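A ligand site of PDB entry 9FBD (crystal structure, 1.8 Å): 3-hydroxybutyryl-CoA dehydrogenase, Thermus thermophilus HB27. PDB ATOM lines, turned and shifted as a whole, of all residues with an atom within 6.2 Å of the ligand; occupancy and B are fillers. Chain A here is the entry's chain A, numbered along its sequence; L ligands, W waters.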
ATOM      1  N   VAL A   9      20.478   4.778 -26.211  1.00  0.00           N
ATOM      2  CA  VAL A   9      19.505   5.910 -26.234  1.00  0.00           C
ATOM      3  C   VAL A   9      19.985   6.955 -25.235  1.00  0.00           C
ATOM      4  O   VAL A   9      20.064   6.662 -24.036  1.00  0.00           O
ATOM      5  CB  VAL A   9      18.059   5.458 -25.985  1.00  0.00           C
ATOM      6  CG1 VAL A   9      17.072   6.574 -26.293  1.00  0.00           C
ATOM      7  CG2 VAL A   9      17.712   4.196 -26.775  1.00  0.00           C
ATOM      8  N   GLY A  10      20.319   8.134 -25.757  1.00  0.00           N
ATOM      9  CA  GLY A  10      20.845   9.268 -25.000  1.00  0.00           C
ATOM     10  C   GLY A  10      22.299   9.461 -25.341  1.00  0.00           C
ATOM     11  O   GLY A  10      23.105   8.598 -24.968  1.00  0.00           O
ATOM     12  N   ALA A  11      22.620  10.559 -26.034  1.00  0.00           N
ATOM     13  CA  ALA A  11      23.991  10.904 -26.456  1.00  0.00           C
ATOM     14  C   ALA A  11      24.538  11.961 -25.495  1.00  0.00           C
ATOM     15  O   ALA A  11      25.235  12.887 -25.969  1.00  0.00           O
ATOM     16  CB  ALA A  11      23.983  11.369 -27.883  1.00  0.00           C
ATOM     17  N   GLY A  12      24.264  11.810 -24.206  1.00  0.00           N
ATOM     18  CA  GLY A  12      24.746  12.714 -23.160  1.00  0.00           C
ATOM     19  C   GLY A  12      26.067  12.233 -22.564  1.00  0.00           C
ATOM     20  O   GLY A  12      26.774  11.437 -23.220  1.00  0.00           O
ATOM     21  N   GLN A  13      26.346  12.708 -21.347  1.00  0.00           N
ATOM     22  CA  GLN A  13      27.611  12.422 -20.600  1.00  0.00           C
ATOM     23  C   GLN A  13      27.839  10.902 -20.572  1.00  0.00           C
ATOM     24  O   GLN A  13      28.965  10.471 -20.856  1.00  0.00           O
ATOM     25  CB  GLN A  13      27.508  13.008 -19.198  1.00  0.00           C
ATOM     26  CG  GLN A  13      28.760  12.793 -18.333  1.00  0.00           C
ATOM     27  CD  GLN A  13      29.985  13.353 -19.002  1.00  0.00           C
ATOM     28  OE1 GLN A  13      29.919  14.306 -19.757  1.00  0.00           O
ATOM     29  NE2 GLN A  13      31.125  12.736 -18.739  1.00  0.00           N
ATOM     30  N   MET A  14      26.822  10.110 -20.250  1.00  0.00           N
ATOM     31  CA  MET A  14      27.001   8.649 -20.038  1.00  0.00           C
ATOM     32  C   MET A  14      26.794   7.901 -21.362  1.00  0.00           C
ATOM     33  O   MET A  14      27.645   7.041 -21.678  1.00  0.00           O
ATOM     34  CB  MET A  14      26.038   8.127 -18.974  1.00  0.00           C
ATOM     35  CG  MET A  14      26.288   8.763 -17.590  1.00  0.00           C
ATOM     36  SD  MET A  14      27.980   8.500 -16.952  1.00  0.00           S
ATOM     37  CE  MET A  14      27.921   6.752 -16.585  1.00  0.00           C
ATOM     38  N   GLY A  15      25.723   8.187 -22.107  1.00  0.00           N
ATOM     39  CA  GLY A  15      25.393   7.470 -23.334  1.00  0.00           C
ATOM     40  C   GLY A  15      26.502   7.548 -24.375  1.00  0.00           C
ATOM     41  O   GLY A  15      26.785   6.547 -25.041  1.00  0.00           O
ATOM     42  N   VAL A  32      21.057   7.069 -30.412  1.00  0.00           N
ATOM     43  CA  VAL A  32      19.765   7.761 -30.651  1.00  0.00           C
ATOM     44  C   VAL A  32      19.609   8.912 -29.666  1.00  0.00           C
ATOM     45  O   VAL A  32      19.926   8.746 -28.469  1.00  0.00           O
ATOM     46  CB  VAL A  32      18.575   6.786 -30.553  1.00  0.00           C
ATOM     47  CG1 VAL A  32      17.248   7.518 -30.804  1.00  0.00           C
ATOM     48  CG2 VAL A  32      18.755   5.602 -31.485  1.00  0.00           C
ATOM     49  N   ASP A  33      19.114  10.050 -30.133  1.00  0.00           N
ATOM     50  CA  ASP A  33      18.737  11.186 -29.264  1.00  0.00           C
ATOM     51  C   ASP A  33      17.547  11.904 -29.932  1.00  0.00           C
ATOM     52  O   ASP A  33      17.002  11.344 -30.894  1.00  0.00           O
ATOM     53  CB  ASP A  33      19.953  12.052 -28.942  1.00  0.00           C
ATOM     54  CG  ASP A  33      19.905  12.769 -27.597  1.00  0.00           C
ATOM     55  OD1 ASP A  33      18.939  13.564 -27.370  1.00  0.00           O
ATOM     56  OD2 ASP A  33      20.823  12.535 -26.782  1.00  0.00           O
ATOM     57  N   VAL A  34      17.150  13.070 -29.409  1.00  0.00           N
ATOM     58  CA  VAL A  34      15.889  13.763 -29.817  1.00  0.00           C
ATOM     59  C   VAL A  34      16.190  14.969 -30.723  1.00  0.00           C
ATOM     60  O   VAL A  34      15.249  15.545 -31.235  1.00  0.00           O
ATOM     61  CB  VAL A  34      15.031  14.171 -28.611  1.00  0.00           C
ATOM     62  CG1 VAL A  34      14.619  12.945 -27.791  1.00  0.00           C
ATOM     63  CG2 VAL A  34      15.710  15.205 -27.741  1.00  0.00           C
ATOM     64  N   ALA A  35      17.444  15.321 -30.948  1.00  0.00           N
ATOM     65  CA  ALA A  35      17.844  16.446 -31.826  1.00  0.00           C
ATOM     66  C   ALA A  35      19.256  16.228 -32.368  1.00  0.00           C
ATOM     67  O   ALA A  35      20.078  15.636 -31.660  1.00  0.00           O
ATOM     68  CB  ALA A  35      17.737  17.776 -31.090  1.00  0.00           C
ATOM     69  N   PHE A  38      22.367  17.395 -30.280  1.00  0.00           N
ATOM     70  CA  PHE A  38      22.700  16.497 -29.144  1.00  0.00           C
ATOM     71  C   PHE A  38      23.567  15.335 -29.664  1.00  0.00           C
ATOM     72  O   PHE A  38      24.541  14.995 -28.970  1.00  0.00           O
ATOM     73  CB  PHE A  38      21.425  16.031 -28.439  1.00  0.00           C
ATOM     74  CG  PHE A  38      20.584  17.137 -27.857  1.00  0.00           C
ATOM     75  CD1 PHE A  38      21.162  18.298 -27.349  1.00  0.00           C
ATOM     76  CD2 PHE A  38      19.206  16.995 -27.754  1.00  0.00           C
ATOM     77  CE1 PHE A  38      20.371  19.310 -26.803  1.00  0.00           C
ATOM     78  CE2 PHE A  38      18.421  17.997 -27.189  1.00  0.00           C
ATOM     79  CZ  PHE A  38      18.999  19.141 -26.705  1.00  0.00           C
ATOM     80  N   ARG A  41      27.016  16.827 -30.379  1.00  0.00           N
ATOM     81  CA  ARG A  41      27.710  17.040 -29.087  1.00  0.00           C
ATOM     82  C   ARG A  41      28.255  15.672 -28.596  1.00  0.00           C
ATOM     83  O   ARG A  41      29.414  15.603 -28.143  1.00  0.00           O
ATOM     84  CB  ARG A  41      26.737  17.709 -28.109  1.00  0.00           C
ATOM     85  CG  ARG A  41      27.297  18.027 -26.731  1.00  0.00           C
ATOM     86  CD  ARG A  41      26.211  18.139 -25.667  1.00  0.00           C
ATOM     87  NE  ARG A  41      25.501  16.875 -25.558  1.00  0.00           N
ATOM     88  CZ  ARG A  41      24.218  16.709 -25.258  1.00  0.00           C
ATOM     89  NH1 ARG A  41      23.701  15.479 -25.248  1.00  0.00           N
ATOM     90  NH2 ARG A  41      23.439  17.733 -25.008  1.00  0.00           N
ATOM     91  N   LEU A  77      13.936   5.792 -33.055  1.00  0.00           N
ATOM     92  CA  LEU A  77      13.969   4.567 -32.207  1.00  0.00           C
ATOM     93  C   LEU A  77      13.767   3.334 -33.080  1.00  0.00           C
ATOM     94  O   LEU A  77      14.324   2.286 -32.725  1.00  0.00           O
ATOM     95  CB  LEU A  77      12.879   4.671 -31.141  1.00  0.00           C
ATOM     96  CG  LEU A  77      13.243   5.547 -29.947  1.00  0.00           C
ATOM     97  CD1 LEU A  77      12.091   5.627 -28.974  1.00  0.00           C
ATOM     98  CD2 LEU A  77      14.517   5.037 -29.243  1.00  0.00           C
ATOM     99  N   GLU A  88      19.705   2.204 -22.310  1.00  0.00           N
ATOM    100  CA  GLU A  88      19.092   3.525 -22.102  1.00  0.00           C
ATOM    101  C   GLU A  88      19.969   4.347 -21.143  1.00  0.00           C
ATOM    102  O   GLU A  88      20.329   3.839 -20.065  1.00  0.00           O
ATOM    103  CB  GLU A  88      17.671   3.336 -21.582  1.00  0.00           C
ATOM    104  CG  GLU A  88      17.050   4.584 -21.026  1.00  0.00           C
ATOM    105  CD  GLU A  88      17.399   4.856 -19.586  1.00  0.00           C
ATOM    106  OE1 GLU A  88      17.844   5.992 -19.281  1.00  0.00           O
ATOM    107  OE2 GLU A  88      17.245   3.925 -18.747  1.00  0.00           O
ATOM    108  N   ALA A  89      20.283   5.566 -21.545  1.00  0.00           N
ATOM    109  CA  ALA A  89      21.017   6.565 -20.745  1.00  0.00           C
ATOM    110  C   ALA A  89      20.404   7.944 -21.010  1.00  0.00           C
ATOM    111  O   ALA A  89      21.139   8.917 -21.304  1.00  0.00           O
ATOM    112  CB  ALA A  89      22.495   6.531 -21.104  1.00  0.00           C
ATOM    113  N   ILE A  90      19.083   8.026 -20.867  1.00  0.00           N
ATOM    114  CA  ILE A  90      18.339   9.306 -21.015  1.00  0.00           C
ATOM    115  C   ILE A  90      18.193   9.946 -19.630  1.00  0.00           C
ATOM    116  O   ILE A  90      18.699   9.363 -18.632  1.00  0.00           O
ATOM    117  CB  ILE A  90      16.992   9.132 -21.735  1.00  0.00           C
ATOM    118  CG1 ILE A  90      15.932   8.397 -20.896  1.00  0.00           C
ATOM    119  CG2 ILE A  90      17.224   8.489 -23.089  1.00  0.00           C
ATOM    120  CD1 ILE A  90      14.518   8.700 -21.334  1.00  0.00           C
ATOM    121  N   VAL A  91      17.550  11.111 -19.602  1.00  0.00           N
ATOM    122  CA  VAL A  91      17.298  11.910 -18.364  1.00  0.00           C
ATOM    123  C   VAL A  91      16.816  10.994 -17.238  1.00  0.00           C
ATOM    124  O   VAL A  91      16.011  10.064 -17.492  1.00  0.00           O
ATOM    125  CB  VAL A  91      16.310  13.071 -18.680  1.00  0.00           C
ATOM    126  CG1 VAL A  91      14.986  12.564 -19.238  1.00  0.00           C
ATOM    127  CG2 VAL A  91      16.063  13.956 -17.463  1.00  0.00           C
ATOM    128  N   GLU A  92      17.255  11.257 -16.014  1.00  0.00           N
ATOM    129  CA  GLU A  92      16.871  10.497 -14.796  1.00  0.00           C
ATOM    130  C   GLU A  92      15.444  10.921 -14.393  1.00  0.00           C
ATOM    131  O   GLU A  92      15.284  11.672 -13.433  1.00  0.00           O
ATOM    132  CB  GLU A  92      17.885  10.748 -13.689  1.00  0.00           C
ATOM    133  CG  GLU A  92      17.686   9.895 -12.446  1.00  0.00           C
ATOM    134  CD  GLU A  92      18.055   8.418 -12.545  1.00  0.00           C
ATOM    135  OE1 GLU A  92      18.021   7.835 -13.669  1.00  0.00           O
ATOM    136  OE2 GLU A  92      18.365   7.838 -11.489  1.00  0.00           O
ATOM    137  N   ASP A  93      14.442  10.483 -15.147  1.00  0.00           N
ATOM    138  CA  ASP A  93      13.009  10.812 -14.910  1.00  0.00           C
ATOM    139  C   ASP A  93      12.207   9.554 -15.211  1.00  0.00           C
ATOM    140  O   ASP A  93      12.294   9.054 -16.343  1.00  0.00           O
ATOM    141  CB  ASP A  93      12.552  11.998 -15.756  1.00  0.00           C
ATOM    142  CG  ASP A  93      11.070  12.296 -15.562  1.00  0.00           C
ATOM    143  OD1 ASP A  93      10.222  11.600 -16.181  1.00  0.00           O
ATOM    144  OD2 ASP A  93      10.783  13.151 -14.742  1.00  0.00           O
ATOM    145  N   GLU A  96       9.710   9.656 -18.257  1.00  0.00           N
ATOM    146  CA  GLU A  96      10.431   9.656 -19.564  1.00  0.00           C
ATOM    147  C   GLU A  96      10.950   8.251 -19.850  1.00  0.00           C
ATOM    148  O   GLU A  96      10.768   7.780 -20.983  1.00  0.00           O
ATOM    149  CB  GLU A  96      11.578  10.664 -19.528  1.00  0.00           C
ATOM    150  CG  GLU A  96      11.145  12.097 -19.698  1.00  0.00           C
ATOM    151  CD  GLU A  96      10.563  12.348 -21.081  1.00  0.00           C
ATOM    152  OE1 GLU A  96      11.311  12.277 -22.095  1.00  0.00           O
ATOM    153  OE2 GLU A  96       9.349  12.528 -21.157  1.00  0.00           O
ATOM    154  N   LYS A  97      11.581   7.599 -18.859  1.00  0.00           N
ATOM    155  CA  LYS A  97      12.137   6.238 -19.071  1.00  0.00           C
ATOM    156  C   LYS A  97      10.970   5.281 -19.323  1.00  0.00           C
ATOM    157  O   LYS A  97      11.096   4.387 -20.180  1.00  0.00           O
ATOM    158  CB  LYS A  97      12.997   5.800 -17.887  1.00  0.00           C
ATOM    159  CG  LYS A  97      14.280   6.574 -17.705  1.00  0.00           C
ATOM    160  CD  LYS A  97      15.260   5.883 -16.771  1.00  0.00           C
ATOM    161  CE  LYS A  97      16.318   6.799 -16.214  1.00  0.00           C
ATOM    162  NZ  LYS A  97      17.169   7.408 -17.264  1.00  0.00           N
ATOM    163  N   LEU A 100       9.798   5.649 -22.885  1.00  0.00           N
ATOM    164  CA  LEU A 100      10.849   5.078 -23.763  1.00  0.00           C
ATOM    165  C   LEU A 100      10.756   3.560 -23.766  1.00  0.00           C
ATOM    166  O   LEU A 100      10.822   2.953 -24.858  1.00  0.00           O
ATOM    167  CB  LEU A 100      12.235   5.537 -23.314  1.00  0.00           C
ATOM    168  CG  LEU A 100      13.408   4.940 -24.079  1.00  0.00           C
ATOM    169  CD1 LEU A 100      13.321   5.319 -25.558  1.00  0.00           C
ATOM    170  CD2 LEU A 100      14.717   5.457 -23.511  1.00  0.00           C
ATOM    171  N   SER A 116      19.006  -0.379 -18.476  1.00  0.00           N
ATOM    172  CA  SER A 116      19.033   1.025 -17.999  1.00  0.00           C
ATOM    173  C   SER A 116      20.341   1.305 -17.261  1.00  0.00           C
ATOM    174  O   SER A 116      20.790   0.461 -16.456  1.00  0.00           O
ATOM    175  CB  SER A 116      17.857   1.319 -17.102  1.00  0.00           C
ATOM    176  OG  SER A 116      17.934   2.664 -16.613  1.00  0.00           O
ATOM    177  N   ASN A 117      20.893   2.482 -17.504  1.00  0.00           N
ATOM    178  CA  ASN A 117      22.044   3.074 -16.791  1.00  0.00           C
ATOM    179  C   ASN A 117      21.551   3.872 -15.564  1.00  0.00           C
ATOM    180  O   ASN A 117      22.349   4.668 -15.025  1.00  0.00           O
ATOM    181  CB  ASN A 117      22.826   3.951 -17.748  1.00  0.00           C
ATOM    182  CG  ASN A 117      24.152   4.404 -17.171  1.00  0.00           C
ATOM    183  OD1 ASN A 117      24.965   3.588 -16.729  1.00  0.00           O
ATOM    184  ND2 ASN A 117      24.366   5.714 -17.183  1.00  0.00           N
ATOM    185  N   THR A 118      20.291   3.760 -15.180  1.00  0.00           N
ATOM    186  CA  THR A 118      19.716   4.614 -14.098  1.00  0.00           C
ATOM    187  C   THR A 118      20.578   4.556 -12.830  1.00  0.00           C
ATOM    188  O   THR A 118      21.095   3.462 -12.466  1.00  0.00           O
ATOM    189  CB  THR A 118      18.271   4.223 -13.787  1.00  0.00           C
ATOM    190  OG1 THR A 118      17.759   5.181 -12.850  1.00  0.00           O
ATOM    191  CG2 THR A 118      18.131   2.820 -13.232  1.00  0.00           C
ATOM    192  N   SER A 119      20.735   5.702 -12.169  1.00  0.00           N
ATOM    193  CA  SER A 119      21.423   5.798 -10.847  1.00  0.00           C
ATOM    194  C   SER A 119      20.522   5.265  -9.739  1.00  0.00           C
ATOM    195  O   SER A 119      21.057   4.783  -8.739  1.00  0.00           O
ATOM    196  CB  SER A 119      21.839   7.197 -10.530  1.00  0.00           C
ATOM    197  OG  SER A 119      22.941   7.568 -11.338  1.00  0.00           O
ATOM    198  N   SER A 120      19.198   5.460  -9.854  1.00  0.00           N
ATOM    199  CA  SER A 120      18.329   5.430  -8.660  1.00  0.00           C
ATOM    200  C   SER A 120      16.934   4.838  -8.915  1.00  0.00           C
ATOM    201  O   SER A 120      16.312   4.413  -7.940  1.00  0.00           O
ATOM    202  CB  SER A 120      18.262   6.812  -8.049  1.00  0.00           C
ATOM    203  OG  SER A 120      17.646   7.761  -8.887  1.00  0.00           O
ATOM    204  N   ILE A 121      16.452   4.768 -10.159  1.00  0.00           N
ATOM    205  CA  ILE A 121      15.059   4.276 -10.432  1.00  0.00           C
ATOM    206  C   ILE A 121      15.052   2.753 -10.359  1.00  0.00           C
ATOM    207  O   ILE A 121      15.917   2.094 -10.913  1.00  0.00           O
ATOM    208  CB  ILE A 121      14.544   4.816 -11.765  1.00  0.00           C
ATOM    209  CG1 ILE A 121      14.486   6.342 -11.730  1.00  0.00           C
ATOM    210  CG2 ILE A 121      13.206   4.194 -12.114  1.00  0.00           C
ATOM    211  CD1 ILE A 121      14.415   7.014 -13.071  1.00  0.00           C
ATOM    212  N   HIS A 140      24.833  -0.386 -15.045  1.00  0.00           N
ATOM    213  CA  HIS A 140      25.162   0.908 -14.404  1.00  0.00           C
ATOM    214  C   HIS A 140      26.654   1.179 -14.577  1.00  0.00           C
ATOM    215  O   HIS A 140      27.491   0.506 -13.930  1.00  0.00           O
ATOM    216  CB  HIS A 140      24.670   0.880 -12.944  1.00  0.00           C
ATOM    217  CG  HIS A 140      24.843   2.163 -12.213  1.00  0.00           C
ATOM    218  ND1 HIS A 140      25.356   2.230 -10.918  1.00  0.00           N
ATOM    219  CD2 HIS A 140      24.572   3.437 -12.582  1.00  0.00           C
ATOM    220  CE1 HIS A 140      25.387   3.477 -10.501  1.00  0.00           C
ATOM    221  NE2 HIS A 140      24.909   4.251 -11.515  1.00  0.00           N
ATOM    222  N   PHE A 141      26.993   2.090 -15.468  1.00  0.00           N
ATOM    223  CA  PHE A 141      28.372   2.500 -15.797  1.00  0.00           C
ATOM    224  C   PHE A 141      28.771   3.643 -14.860  1.00  0.00           C
ATOM    225  O   PHE A 141      27.896   4.211 -14.179  1.00  0.00           O
ATOM    226  CB  PHE A 141      28.486   2.902 -17.265  1.00  0.00           C
ATOM    227  CG  PHE A 141      28.309   1.777 -18.261  1.00  0.00           C
ATOM    228  CD1 PHE A 141      27.038   1.356 -18.636  1.00  0.00           C
ATOM    229  CD2 PHE A 141      29.407   1.143 -18.823  1.00  0.00           C
ATOM    230  CE1 PHE A 141      26.881   0.349 -19.578  1.00  0.00           C
ATOM    231  CE2 PHE A 141      29.250   0.145 -19.775  1.00  0.00           C
ATOM    232  CZ  PHE A 141      27.981  -0.253 -20.149  1.00  0.00           C
ATOM    233  N   PHE A 142      30.062   3.974 -14.852  1.00  0.00           N
ATOM    234  CA  PHE A 142      30.664   5.006 -13.972  1.00  0.00           C
ATOM    235  C   PHE A 142      31.316   6.077 -14.850  1.00  0.00           C
ATOM    236  O   PHE A 142      31.891   5.776 -15.906  1.00  0.00           O
ATOM    237  CB  PHE A 142      31.577   4.310 -12.965  1.00  0.00           C
ATOM    238  CG  PHE A 142      30.798   3.610 -11.894  1.00  0.00           C
ATOM    239  CD1 PHE A 142      30.113   2.445 -12.176  1.00  0.00           C
ATOM    240  CD2 PHE A 142      30.641   4.199 -10.645  1.00  0.00           C
ATOM    241  CE1 PHE A 142      29.327   1.850 -11.210  1.00  0.00           C
ATOM    242  CE2 PHE A 142      29.850   3.596  -9.676  1.00  0.00           C
ATOM    243  CZ  PHE A 142      29.202   2.432  -9.968  1.00  0.00           C
ATOM    244  N   ASN A 143      31.153   7.305 -14.414  1.00  0.00           N
ATOM    245  CA  ASN A 143      31.540   8.546 -15.136  1.00  0.00           C
ATOM    246  C   ASN A 143      33.015   8.833 -14.856  1.00  0.00           C
ATOM    247  O   ASN A 143      33.408   8.895 -13.700  1.00  0.00           O
ATOM    248  CB  ASN A 143      30.665   9.705 -14.646  1.00  0.00           C
ATOM    249  CG  ASN A 143      30.843  10.970 -15.442  1.00  0.00           C
ATOM    250  OD1 ASN A 143      31.632  11.025 -16.378  1.00  0.00           O
ATOM    251  ND2 ASN A 143      30.067  11.983 -15.090  1.00  0.00           N
HETATM  252  P1  LIG L   1      22.646  13.798 -19.935  1.00  0.00           P
HETATM  253  O1  LIG L   1      21.607  14.851 -19.716  1.00  0.00           O
HETATM  254  O2  LIG L   1      24.072  14.210 -20.105  1.00  0.00           O
HETATM  255  O3  LIG L   1      22.173  12.942 -21.192  1.00  0.00           O
HETATM  256  C1  LIG L   1      20.793  12.564 -21.441  1.00  0.00           C
HETATM  257  C2  LIG L   1      20.549  12.563 -22.924  1.00  0.00           C
HETATM  258  O4  LIG L   1      19.266  11.943 -23.143  1.00  0.00           O
HETATM  259  C3  LIG L   1      20.494  13.936 -23.645  1.00  0.00           C
HETATM  260  O5  LIG L   1      21.310  13.907 -24.812  1.00  0.00           O
HETATM  261  C4  LIG L   1      19.006  14.109 -24.014  1.00  0.00           C
HETATM  262  O6  LIG L   1      18.839  14.765 -25.253  1.00  0.00           O
HETATM  263  C5  LIG L   1      18.593  12.648 -24.151  1.00  0.00           C
HETATM  264  N1  LIG L   1      17.174  12.335 -23.990  1.00  0.00           N
HETATM  265  C6  LIG L   1      16.318  12.770 -23.004  1.00  0.00           C
HETATM  266  N2  LIG L   1      15.111  12.253 -23.109  1.00  0.00           N
HETATM  267  C7  LIG L   1      15.202  11.402 -24.198  1.00  0.00           C
HETATM  268  C8  LIG L   1      14.266  10.561 -24.798  1.00  0.00           C
HETATM  269  N3  LIG L   1      13.016  10.448 -24.350  1.00  0.00           N
HETATM  270  N4  LIG L   1      14.676   9.816 -25.845  1.00  0.00           N
HETATM  271  C9  LIG L   1      15.925   9.966 -26.290  1.00  0.00           C
HETATM  272  N5  LIG L   1      16.905  10.724 -25.791  1.00  0.00           N
HETATM  273  C10 LIG L   1      16.471  11.435 -24.743  1.00  0.00           C
HETATM  274  O7  LIG L   1      22.536  12.754 -18.711  1.00  0.00           O
HETATM  275  P2  LIG L   1      23.616  11.693 -18.164  1.00  0.00           P
HETATM  276  O8  LIG L   1      24.422  12.295 -17.120  1.00  0.00           O
HETATM  277  O9  LIG L   1      24.232  11.104 -19.403  1.00  0.00           O
HETATM  278  O10 LIG L   1      22.663  10.628 -17.445  1.00  0.00           O
HETATM  279  C11 LIG L   1      21.985   9.655 -18.207  1.00  0.00           C
HETATM  280  C12 LIG L   1      21.497   8.563 -17.287  1.00  0.00           C
HETATM  281  O11 LIG L   1      22.643   7.944 -16.644  1.00  0.00           O
HETATM  282  C13 LIG L   1      20.574   9.006 -16.133  1.00  0.00           C
HETATM  283  O12 LIG L   1      19.620   7.975 -15.841  1.00  0.00           O
HETATM  284  C14 LIG L   1      21.552   9.187 -14.964  1.00  0.00           C
HETATM  285  O13 LIG L   1      20.954   8.974 -13.686  1.00  0.00           O
HETATM  286  C15 LIG L   1      22.506   8.007 -15.223  1.00  0.00           C
HETATM  287  N6  LIG L   1      23.844   8.153 -14.593  1.00  0.00           N
HETATM  288  C16 LIG L   1      24.548   9.353 -14.644  1.00  0.00           C
HETATM  289  C17 LIG L   1      25.815   9.439 -14.082  1.00  0.00           C
HETATM  290  C18 LIG L   1      26.614  10.712 -14.149  1.00  0.00           C
HETATM  291  O14 LIG L   1      27.541  10.850 -13.359  1.00  0.00           O
HETATM  292  N7  LIG L   1      26.331  11.607 -15.094  1.00  0.00           N
HETATM  293  C19 LIG L   1      26.373   8.310 -13.442  1.00  0.00           C
HETATM  294  C20 LIG L   1      25.722   7.085 -13.562  1.00  0.00           C
HETATM  295  C21 LIG L   1      24.433   7.058 -14.027  1.00  0.00           C
HETATM  296  O   HOH W   1      20.491  16.969 -24.537  1.00  0.00           O
HETATM  297  O   HOH W   2      16.740  16.514 -24.329  1.00  0.00           O
HETATM  298  O   HOH W   3      27.448  14.334 -15.166  1.00  0.00           O
HETATM  299  O   HOH W   4      25.195  16.401 -21.310  1.00  0.00           O
HETATM  300  O   HOH W   5      23.503  10.034 -21.803  1.00  0.00           O
HETATM  301  O   HOH W   6      19.636  14.630 -18.213  1.00  0.00           O
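The backbone carbonyl oxygen (O) of Ile 90 lies close to an oxygen (O12) of the ligand (3.3 Å). O9 of the ligand sits at hydrogen-bond distance from N of Met 14, at 2.9 Å. The guanidinium group of Arg 41 sits at hydrogen-bond distance from an oxygen (O5) of the ligand, at 2.9 Å. O13 of the ligand lies close to OG of Ser 119 (3.4 Å). The backbone NH (N) of Gln 13 is in hydrogen-bond range of an oxygen (O2) of the ligand (3.0 Å). The side-chain carboxylate (OD1) of Asp 33 lies within hydrogen-bond range of an oxygen (O6) of the ligand (2.4 Å). The side-chain carboxylate of Glu 92 lies within hydrogen-bond range of an oxygen (O12) of the ligand, at 2.7 Å. OE1 of Glu 96 sits at hydrogen-bond distance from N3 of the ligand. O12 of the ligand sits at hydrogen-bond distance from NZ of Lys 97. O14 of the ligand lies within hydrogen-bond range of ND2 of Asn 143. The side-chain amide nitrogen (ND2) of Asn 117 lies within hydrogen-bond range of an oxygen (O11) of the ligand, 2.9 Å away.
N of Phe 141 sits at hydrogen-bond distance from OD1 of Asn 117. The side-chain amide oxygen of Asn 143 lies within hydrogen-bond range of the side-chain amide nitrogen of Gln 13, at 3.0 Å. The side-chain hydroxyl (OG) of Ser 120 lies within hydrogen-bond range of the side-chain carboxylate (OE2) of Glu 92. The backbone NH (N) of Ser 119 is in hydrogen-bond range of the side-chain carboxylate (OE2) of Glu 92, 3.3 Å away. The side-chain amino group of Lys 97 is in hydrogen-bond range of the backbone carbonyl oxygen of Val 91 (2.9 Å). N of Ala 89 sits at hydrogen-bond distance from O of Val 9 (2.7 Å). The side-chain carboxylate of Glu 88 is in salt-bridge range of the side-chain amino group of Lys 97 (2.6 Å). The side-chain carboxylate of Glu 92 is in hydrogen-bond range of the side-chain hydroxyl of Thr 118, at 2.8 Å.
Val 9 touches the ligand (CG1 to C9, 3.6 Å). Gly 10 touches the ligand. Ala 11 touches the ligand (N to O5, 3.8 Å). Gly 12 touches the ligand. Val 34 touches the ligand (CG1 to C9, 3.6 Å). Phe 38 touches the ligand (CD2 to O6, 3.4 Å). O of Ala 89 touches C11 of the ligand, at 3.3 Å. Val 91 touches the ligand (CG1 to N2, 3.9 Å). Thr 118 touches the ligand (CA to O12, 3.8 Å). His 140 touches the ligand (NE2 to C20, 3.6 Å). Phe 141 touches the ligand (O to C20, 3.7 Å). 22 residues have an atom within 4 Å of the ligand: Val 9, Gly 10, Ala 11, Gly 12, Gln 13, Met 14, Asp 33, Val 34, Phe 38, Arg 41, Ala 89, Ile 90, Val 91, Glu 92, Glu 96, Lys 97, Asn 117, Thr 118, Ser 119, His 140, Phe 141 and Asn 143.
Water W5 lies within hydrogen-bond range of O of Ala 89 (2.7 Å), O9 of the ligand (2.7 Å), N of Gly 15 (2.9 Å), N of Gly 12 (3.1 Å) and O of Gly 10 (3.5 Å). Water W1 bridges an oxygen (O6) of the ligand and the guanidinium group of Arg 41.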
